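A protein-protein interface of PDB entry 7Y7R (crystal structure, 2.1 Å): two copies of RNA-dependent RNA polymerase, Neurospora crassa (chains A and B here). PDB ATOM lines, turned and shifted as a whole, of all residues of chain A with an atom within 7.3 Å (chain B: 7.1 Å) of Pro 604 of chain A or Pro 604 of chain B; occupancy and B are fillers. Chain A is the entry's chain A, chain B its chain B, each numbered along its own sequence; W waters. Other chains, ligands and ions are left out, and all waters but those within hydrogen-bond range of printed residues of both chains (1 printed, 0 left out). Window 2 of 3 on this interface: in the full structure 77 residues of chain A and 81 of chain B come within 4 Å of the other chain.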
ATOM      1  N   VAL A 553     -20.804  -0.823   1.579  1.00  0.00           N
ATOM      2  CA  VAL A 553     -20.379   0.511   1.164  1.00  0.00           C
ATOM      3  C   VAL A 553     -20.809   1.619   2.122  1.00  0.00           C
ATOM      4  O   VAL A 553     -20.168   2.682   2.151  1.00  0.00           O
ATOM      5  CB  VAL A 553     -20.890   0.828  -0.250  1.00  0.00           C
ATOM      6  CG1 VAL A 553     -20.164  -0.049  -1.255  1.00  0.00           C
ATOM      7  CG2 VAL A 553     -22.410   0.634  -0.340  1.00  0.00           C
ATOM      8  N   HIS A 560     -28.531   5.462   2.569  1.00  0.00           N
ATOM      9  CA  HIS A 560     -28.631   5.702   1.135  1.00  0.00           C
ATOM     10  C   HIS A 560     -30.103   5.761   0.759  1.00  0.00           C
ATOM     11  O   HIS A 560     -30.855   4.840   1.082  1.00  0.00           O
ATOM     12  CB  HIS A 560     -27.920   4.589   0.348  1.00  0.00           C
ATOM     13  CG  HIS A 560     -28.130   4.648  -1.141  1.00  0.00           C
ATOM     14  ND1 HIS A 560     -27.142   5.056  -2.016  1.00  0.00           N
ATOM     15  CD2 HIS A 560     -29.195   4.307  -1.910  1.00  0.00           C
ATOM     16  CE1 HIS A 560     -27.599   4.987  -3.254  1.00  0.00           C
ATOM     17  NE2 HIS A 560     -28.845   4.542  -3.219  1.00  0.00           N
ATOM     18  N   LEU A 576     -32.665  11.912  -5.241  1.00  0.00           N
ATOM     19  CA  LEU A 576     -31.875  11.171  -4.266  1.00  0.00           C
ATOM     20  C   LEU A 576     -31.581  12.117  -3.107  1.00  0.00           C
ATOM     21  O   LEU A 576     -31.853  13.316  -3.181  1.00  0.00           O
ATOM     22  CB  LEU A 576     -30.582  10.624  -4.884  1.00  0.00           C
ATOM     23  CG  LEU A 576     -29.673  11.688  -5.525  1.00  0.00           C
ATOM     24  CD1 LEU A 576     -28.725  12.292  -4.513  1.00  0.00           C
ATOM     25  CD2 LEU A 576     -28.863  11.120  -6.673  1.00  0.00           C
ATOM     26  N   SER A 578     -28.407  13.390  -0.661  1.00  0.00           N
ATOM     27  CA  SER A 578     -26.958  13.371  -0.590  1.00  0.00           C
ATOM     28  C   SER A 578     -26.507  14.519   0.298  1.00  0.00           C
ATOM     29  O   SER A 578     -27.128  15.584   0.303  1.00  0.00           O
ATOM     30  CB  SER A 578     -26.340  13.484  -1.986  1.00  0.00           C
ATOM     31  OG  SER A 578     -24.930  13.490  -1.917  1.00  0.00           O
ATOM     32  N   ASP A 579     -25.446  14.277   1.068  1.00  0.00           N
ATOM     33  CA  ASP A 579     -24.786  15.298   1.881  1.00  0.00           C
ATOM     34  C   ASP A 579     -25.781  16.139   2.681  1.00  0.00           C
ATOM     35  O   ASP A 579     -25.763  17.369   2.652  1.00  0.00           O
ATOM     36  CB  ASP A 579     -23.897  16.188   1.010  1.00  0.00           C
ATOM     37  CG  ASP A 579     -22.426  15.821   1.117  1.00  0.00           C
ATOM     38  OD1 ASP A 579     -21.926  15.655   2.254  1.00  0.00           O
ATOM     39  OD2 ASP A 579     -21.764  15.710   0.064  1.00  0.00           O
ATOM     40  N   VAL A 601     -25.900   9.564   2.490  1.00  0.00           N
ATOM     41  CA  VAL A 601     -24.770   9.496   1.569  1.00  0.00           C
ATOM     42  C   VAL A 601     -25.194   8.659   0.375  1.00  0.00           C
ATOM     43  O   VAL A 601     -25.532   7.482   0.535  1.00  0.00           O
ATOM     44  CB  VAL A 601     -23.534   8.869   2.229  1.00  0.00           C
ATOM     45  CG1 VAL A 601     -22.378   8.820   1.244  1.00  0.00           C
ATOM     46  CG2 VAL A 601     -23.170   9.650   3.488  1.00  0.00           C
ATOM     47  N   PHE A 602     -25.159   9.241  -0.820  1.00  0.00           N
ATOM     48  CA  PHE A 602     -25.569   8.490  -2.001  1.00  0.00           C
ATOM     49  C   PHE A 602     -24.380   7.699  -2.543  1.00  0.00           C
ATOM     50  O   PHE A 602     -23.380   8.277  -2.977  1.00  0.00           O
ATOM     51  CB  PHE A 602     -26.155   9.413  -3.060  1.00  0.00           C
ATOM     52  CG  PHE A 602     -26.801   8.675  -4.204  1.00  0.00           C
ATOM     53  CD1 PHE A 602     -28.117   8.244  -4.117  1.00  0.00           C
ATOM     54  CD2 PHE A 602     -26.085   8.397  -5.358  1.00  0.00           C
ATOM     55  CE1 PHE A 602     -28.712   7.575  -5.163  1.00  0.00           C
ATOM     56  CE2 PHE A 602     -26.675   7.720  -6.414  1.00  0.00           C
ATOM     57  CZ  PHE A 602     -27.986   7.308  -6.319  1.00  0.00           C
ATOM     58  N   LYS A 603     -24.475   6.376  -2.506  1.00  0.00           N
ATOM     59  CA  LYS A 603     -23.410   5.533  -3.029  1.00  0.00           C
ATOM     60  C   LYS A 603     -23.755   5.131  -4.454  1.00  0.00           C
ATOM     61  O   LYS A 603     -24.811   4.513  -4.675  1.00  0.00           O
ATOM     62  CB  LYS A 603     -23.227   4.300  -2.152  1.00  0.00           C
ATOM     63  CG  LYS A 603     -23.003   4.634  -0.679  1.00  0.00           C
ATOM     64  CD  LYS A 603     -21.607   5.242  -0.452  1.00  0.00           C
ATOM     65  CE  LYS A 603     -21.348   5.539   1.023  1.00  0.00           C
ATOM     66  NZ  LYS A 603     -19.895   5.664   1.352  1.00  0.00           N
ATOM     67  N   PRO A 604     -22.938   5.481  -5.454  1.00  0.00           N
ATOM     68  CA  PRO A 604     -23.295   5.104  -6.828  1.00  0.00           C
ATOM     69  C   PRO A 604     -23.440   3.602  -7.021  1.00  0.00           C
ATOM     70  O   PRO A 604     -24.225   3.180  -7.884  1.00  0.00           O
ATOM     71  CB  PRO A 604     -22.149   5.701  -7.660  1.00  0.00           C
ATOM     72  CG  PRO A 604     -21.685   6.875  -6.837  1.00  0.00           C
ATOM     73  CD  PRO A 604     -21.788   6.406  -5.412  1.00  0.00           C
ATOM     74  N   GLU A 605     -22.734   2.782  -6.231  1.00  0.00           N
ATOM     75  CA  GLU A 605     -22.899   1.327  -6.301  1.00  0.00           C
ATOM     76  C   GLU A 605     -24.350   0.905  -6.116  1.00  0.00           C
ATOM     77  O   GLU A 605     -24.793  -0.087  -6.715  1.00  0.00           O
ATOM     78  CB  GLU A 605     -22.047   0.637  -5.231  1.00  0.00           C
ATOM     79  CG  GLU A 605     -20.589   1.026  -5.231  1.00  0.00           C
ATOM     80  CD  GLU A 605     -20.323   2.251  -4.384  1.00  0.00           C
ATOM     81  OE1 GLU A 605     -19.445   2.189  -3.491  1.00  0.00           O
ATOM     82  OE2 GLU A 605     -20.992   3.281  -4.626  1.00  0.00           O
ATOM     83  N   LEU A 606     -25.093   1.618  -5.267  1.00  0.00           N
ATOM     84  CA  LEU A 606     -26.460   1.264  -4.924  1.00  0.00           C
ATOM     85  C   LEU A 606     -27.499   2.010  -5.758  1.00  0.00           C
ATOM     86  O   LEU A 606     -28.704   1.838  -5.529  1.00  0.00           O
ATOM     87  CB  LEU A 606     -26.702   1.513  -3.436  1.00  0.00           C
ATOM     88  CG  LEU A 606     -25.647   0.909  -2.508  1.00  0.00           C
ATOM     89  CD1 LEU A 606     -25.934   1.269  -1.068  1.00  0.00           C
ATOM     90  CD2 LEU A 606     -25.576  -0.595  -2.673  1.00  0.00           C
ATOM     91  N   HIS A 607     -27.062   2.808  -6.737  1.00  0.00           N
ATOM     92  CA  HIS A 607     -27.982   3.679  -7.468  1.00  0.00           C
ATOM     93  C   HIS A 607     -29.182   2.934  -8.030  1.00  0.00           C
ATOM     94  O   HIS A 607     -30.235   3.541  -8.260  1.00  0.00           O
ATOM     95  CB  HIS A 607     -27.254   4.374  -8.625  1.00  0.00           C
ATOM     96  CG  HIS A 607     -27.123   3.517  -9.842  1.00  0.00           C
ATOM     97  ND1 HIS A 607     -26.057   2.666 -10.039  1.00  0.00           N
ATOM     98  CD2 HIS A 607     -27.938   3.355 -10.913  1.00  0.00           C
ATOM     99  CE1 HIS A 607     -26.214   2.023 -11.184  1.00  0.00           C
ATOM    100  NE2 HIS A 607     -27.345   2.426 -11.736  1.00  0.00           N
ATOM    101  N   SER A 608     -29.047   1.643  -8.312  1.00  0.00           N
ATOM    102  CA  SER A 608     -30.194   0.953  -8.894  1.00  0.00           C
ATOM    103  C   SER A 608     -31.262   0.565  -7.872  1.00  0.00           C
ATOM    104  O   SER A 608     -32.349   0.139  -8.275  1.00  0.00           O
ATOM    105  CB  SER A 608     -29.729  -0.287  -9.648  1.00  0.00           C
ATOM    106  OG  SER A 608     -29.508  -1.334  -8.733  1.00  0.00           O
ATOM    107  N   HIS B 560     -20.897  12.800 -16.827  1.00  0.00           N
ATOM    108  CA  HIS B 560     -21.869  12.711 -15.748  1.00  0.00           C
ATOM    109  C   HIS B 560     -23.240  13.134 -16.268  1.00  0.00           C
ATOM    110  O   HIS B 560     -23.377  14.211 -16.853  1.00  0.00           O
ATOM    111  CB  HIS B 560     -21.455  13.592 -14.565  1.00  0.00           C
ATOM    112  CG  HIS B 560     -22.503  13.687 -13.497  1.00  0.00           C
ATOM    113  ND1 HIS B 560     -22.405  13.017 -12.294  1.00  0.00           N
ATOM    114  CD2 HIS B 560     -23.689  14.345 -13.467  1.00  0.00           C
ATOM    115  CE1 HIS B 560     -23.473  13.282 -11.561  1.00  0.00           C
ATOM    116  NE2 HIS B 560     -24.269  14.082 -12.249  1.00  0.00           N
ATOM    117  N   LEU B 576     -30.580   8.679 -13.505  1.00  0.00           N
ATOM    118  CA  LEU B 576     -29.204   9.080 -13.769  1.00  0.00           C
ATOM    119  C   LEU B 576     -28.594   8.002 -14.661  1.00  0.00           C
ATOM    120  O   LEU B 576     -29.197   6.952 -14.884  1.00  0.00           O
ATOM    121  CB  LEU B 576     -28.410   9.250 -12.464  1.00  0.00           C
ATOM    122  CG  LEU B 576     -28.356   8.053 -11.494  1.00  0.00           C
ATOM    123  CD1 LEU B 576     -27.257   7.110 -11.908  1.00  0.00           C
ATOM    124  CD2 LEU B 576     -28.091   8.523 -10.073  1.00  0.00           C
ATOM    125  N   SER B 578     -25.144   5.580 -14.926  1.00  0.00           N
ATOM    126  CA  SER B 578     -24.005   5.155 -14.125  1.00  0.00           C
ATOM    127  C   SER B 578     -23.445   3.845 -14.660  1.00  0.00           C
ATOM    128  O   SER B 578     -24.200   2.953 -15.055  1.00  0.00           O
ATOM    129  CB  SER B 578     -24.394   4.988 -12.655  1.00  0.00           C
ATOM    130  OG  SER B 578     -23.250   4.793 -11.845  1.00  0.00           O
ATOM    131  N   ASP B 579     -22.117   3.746 -14.671  1.00  0.00           N
ATOM    132  CA  ASP B 579     -21.398   2.517 -15.004  1.00  0.00           C
ATOM    133  C   ASP B 579     -21.909   1.885 -16.296  1.00  0.00           C
ATOM    134  O   ASP B 579     -22.327   0.726 -16.336  1.00  0.00           O
ATOM    135  CB  ASP B 579     -21.470   1.517 -13.851  1.00  0.00           C
ATOM    136  CG  ASP B 579     -20.249   1.574 -12.967  1.00  0.00           C
ATOM    137  OD1 ASP B 579     -19.653   2.671 -12.860  1.00  0.00           O
ATOM    138  OD2 ASP B 579     -19.881   0.526 -12.392  1.00  0.00           O
ATOM    139  N   VAL B 601     -20.271   8.086 -15.712  1.00  0.00           N
ATOM    140  CA  VAL B 601     -19.905   7.872 -14.319  1.00  0.00           C
ATOM    141  C   VAL B 601     -20.647   8.916 -13.504  1.00  0.00           C
ATOM    142  O   VAL B 601     -20.497  10.116 -13.749  1.00  0.00           O
ATOM    143  CB  VAL B 601     -18.387   7.996 -14.104  1.00  0.00           C
ATOM    144  CG1 VAL B 601     -18.046   7.870 -12.644  1.00  0.00           C
ATOM    145  CG2 VAL B 601     -17.645   6.945 -14.924  1.00  0.00           C
ATOM    146  N   PHE B 602     -21.442   8.475 -12.542  1.00  0.00           N
ATOM    147  CA  PHE B 602     -22.191   9.412 -11.717  1.00  0.00           C
ATOM    148  C   PHE B 602     -21.347   9.844 -10.515  1.00  0.00           C
ATOM    149  O   PHE B 602     -20.935   9.007  -9.707  1.00  0.00           O
ATOM    150  CB  PHE B 602     -23.505   8.783 -11.272  1.00  0.00           C
ATOM    151  CG  PHE B 602     -24.424   9.746 -10.590  1.00  0.00           C
ATOM    152  CD1 PHE B 602     -25.319  10.506 -11.319  1.00  0.00           C
ATOM    153  CD2 PHE B 602     -24.367   9.909  -9.214  1.00  0.00           C
ATOM    154  CE1 PHE B 602     -26.163  11.396 -10.692  1.00  0.00           C
ATOM    155  CE2 PHE B 602     -25.199  10.789  -8.583  1.00  0.00           C
ATOM    156  CZ  PHE B 602     -26.105  11.532  -9.314  1.00  0.00           C
ATOM    157  N   LYS B 603     -21.085  11.149 -10.405  1.00  0.00           N
ATOM    158  CA  LYS B 603     -20.276  11.702  -9.319  1.00  0.00           C
ATOM    159  C   LYS B 603     -21.179  12.406  -8.316  1.00  0.00           C
ATOM    160  O   LYS B 603     -21.790  13.434  -8.657  1.00  0.00           O
ATOM    161  CB  LYS B 603     -19.228  12.680  -9.855  1.00  0.00           C
ATOM    162  CG  LYS B 603     -18.563  12.234 -11.130  1.00  0.00           C
ATOM    163  CD  LYS B 603     -17.742  10.991 -10.901  1.00  0.00           C
ATOM    164  CE  LYS B 603     -16.623  11.257  -9.913  1.00  0.00           C
ATOM    165  NZ  LYS B 603     -15.415  10.448 -10.260  1.00  0.00           N
ATOM    166  N   PRO B 604     -21.321  11.892  -7.094  1.00  0.00           N
ATOM    167  CA  PRO B 604     -22.205  12.558  -6.121  1.00  0.00           C
ATOM    168  C   PRO B 604     -21.906  14.036  -5.928  1.00  0.00           C
ATOM    169  O   PRO B 604     -22.841  14.818  -5.703  1.00  0.00           O
ATOM    170  CB  PRO B 604     -21.983  11.743  -4.841  1.00  0.00           C
ATOM    171  CG  PRO B 604     -21.667  10.359  -5.361  1.00  0.00           C
ATOM    172  CD  PRO B 604     -20.875  10.564  -6.634  1.00  0.00           C
ATOM    173  N   GLU B 605     -20.644  14.453  -6.059  1.00  0.00           N
ATOM    174  CA  GLU B 605     -20.319  15.883  -6.077  1.00  0.00           C
ATOM    175  C   GLU B 605     -21.175  16.663  -7.073  1.00  0.00           C
ATOM    176  O   GLU B 605     -21.474  17.840  -6.846  1.00  0.00           O
ATOM    177  CB  GLU B 605     -18.843  16.081  -6.426  1.00  0.00           C
ATOM    178  CG  GLU B 605     -17.891  15.228  -5.598  1.00  0.00           C
ATOM    179  CD  GLU B 605     -17.748  13.808  -6.138  1.00  0.00           C
ATOM    180  OE1 GLU B 605     -18.775  13.086  -6.234  1.00  0.00           O
ATOM    181  OE2 GLU B 605     -16.604  13.411  -6.456  1.00  0.00           O
ATOM    182  N   LEU B 606     -21.567  16.038  -8.185  1.00  0.00           N
ATOM    183  CA  LEU B 606     -22.328  16.716  -9.223  1.00  0.00           C
ATOM    184  C   LEU B 606     -23.817  16.402  -9.158  1.00  0.00           C
ATOM    185  O   LEU B 606     -24.566  16.827 -10.047  1.00  0.00           O
ATOM    186  CB  LEU B 606     -21.758  16.367 -10.608  1.00  0.00           C
ATOM    187  CG  LEU B 606     -20.238  16.536 -10.724  1.00  0.00           C
ATOM    188  CD1 LEU B 606     -19.696  16.207 -12.117  1.00  0.00           C
ATOM    189  CD2 LEU B 606     -19.827  17.932 -10.326  1.00  0.00           C
ATOM    190  N   HIS B 607     -24.265  15.709  -8.102  1.00  0.00           N
ATOM    191  CA  HIS B 607     -25.628  15.183  -8.067  1.00  0.00           C
ATOM    192  C   HIS B 607     -26.669  16.273  -8.270  1.00  0.00           C
ATOM    193  O   HIS B 607     -27.754  15.997  -8.789  1.00  0.00           O
ATOM    194  CB  HIS B 607     -25.885  14.451  -6.743  1.00  0.00           C
ATOM    195  CG  HIS B 607     -26.223  15.361  -5.606  1.00  0.00           C
ATOM    196  ND1 HIS B 607     -25.274  15.840  -4.723  1.00  0.00           N
ATOM    197  CD2 HIS B 607     -27.405  15.890  -5.210  1.00  0.00           C
ATOM    198  CE1 HIS B 607     -25.857  16.623  -3.833  1.00  0.00           C
ATOM    199  NE2 HIS B 607     -27.150  16.673  -4.108  1.00  0.00           N
ATOM    200  N   SER B 608     -26.373  17.507  -7.877  1.00  0.00           N
ATOM    201  CA  SER B 608     -27.374  18.558  -8.000  1.00  0.00           C
ATOM    202  C   SER B 608     -27.477  19.166  -9.405  1.00  0.00           C
ATOM    203  O   SER B 608     -28.355  20.012  -9.627  1.00  0.00           O
ATOM    204  CB  SER B 608     -27.094  19.666  -6.974  1.00  0.00           C
ATOM    205  OG  SER B 608     -25.961  20.436  -7.345  1.00  0.00           O
HETATM  206  O   HOH W   1     -23.075   2.150 -10.505  1.00  0.00           O
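O of Pro 604 of chain A is in hydrogen-bond range of ND1 of His 607 of chain A, 2.9 Å away.
The backbone carbonyl oxygen (O) of Pro 604 of chain B lies within hydrogen-bond range of a ring nitrogen (ND1) of His 607 of chain B (2.8 Å).
Among the printed residues, merely in contact across the chains: Leu 576 of chain A with Phe 602 of chain B, Leu 576 of chain A with His 607 of chain B, Ser 578 of chain A with His 607 of chain B, Phe 602 of chain A with Leu 576 of chain B, Phe 602 of chain A with Pro 604 of chain B, Pro 604 of chain A with Phe 602 of chain B, Pro 604 of chain A with Pro 604 of chain B, His 607 of chain A with Leu 576 of chain B and His 607 of chain A with Ser 578 of chain B.
Pro 604 of chain A touches just these residues of chain B: Phe 602 and Pro 604.
Pro 604 of chain B touches just these residues of chain A: Phe 602 (3.6 Å) and Pro 604 (3.8 Å).
Of the printed residues of chain A, Ser 578 of chain B touches His 607 (3.8 Å).
Printed residues of chain B within 4 Å of Ser 578 of chain A: His 607.
Printed residues of chain B within 4 Å of Phe 602 of chain A: Leu 576 (3.9 Å) and Pro 604 (3.6 Å).
Ser 608 of chain B touches none of the printed residues of chain A.
Asp 579 of chain B touches none of the printed residues of chain A.
The nearest residue of chain A that does not touch Pro 604 of chain B is Ser 578 of chain A (4.5 Å).
Hydrophobic or aromatic side chains of chain A within 4 Å of the printed part of chain B: Leu 576, Phe 602, Pro 604 and His 607.
Of the 12 printed residues of chain B, 5 touch a printed residue of chain A.
Hydrophobic or aromatic side chains of chain B within 4 Å of the printed part of chain A: Leu 576, Phe 602, Pro 604 and His 607.
Among the printed residues, no Asp or Glu carboxylate lies within 4 Å of a Lys or Arg side-chain nitrogen of the other chain.
Leu 576 of chain A touches His 607 of chain B, and with the chains exchanged His 607 of chain A touches Leu 576 of chain B.
Ser 578 of chain A touches His 607 of chain B, and with the chains exchanged His 607 of chain A touches Ser 578 of chain B.
Phe 602 of chain A touches Pro 604 of chain B, and with the chains exchanged Pro 604 of chain A touches Phe 602 of chain B.
Pro 604 of chain B touches its own counterpart, Pro 604 of chain A.
Of the 9 pairs that touch across the chains among the printed residues, 9 have their exchanged pair printed and touching as well.
Water W1 lies within hydrogen-bond range of the side-chain hydroxyl of Ser 578 of chain B (3.0 Å), the backbone carbonyl oxygen of Pro 604 of chain A (3.0 Å) and a ring nitrogen (ND1) of His 607 of chain A (3.1 Å).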
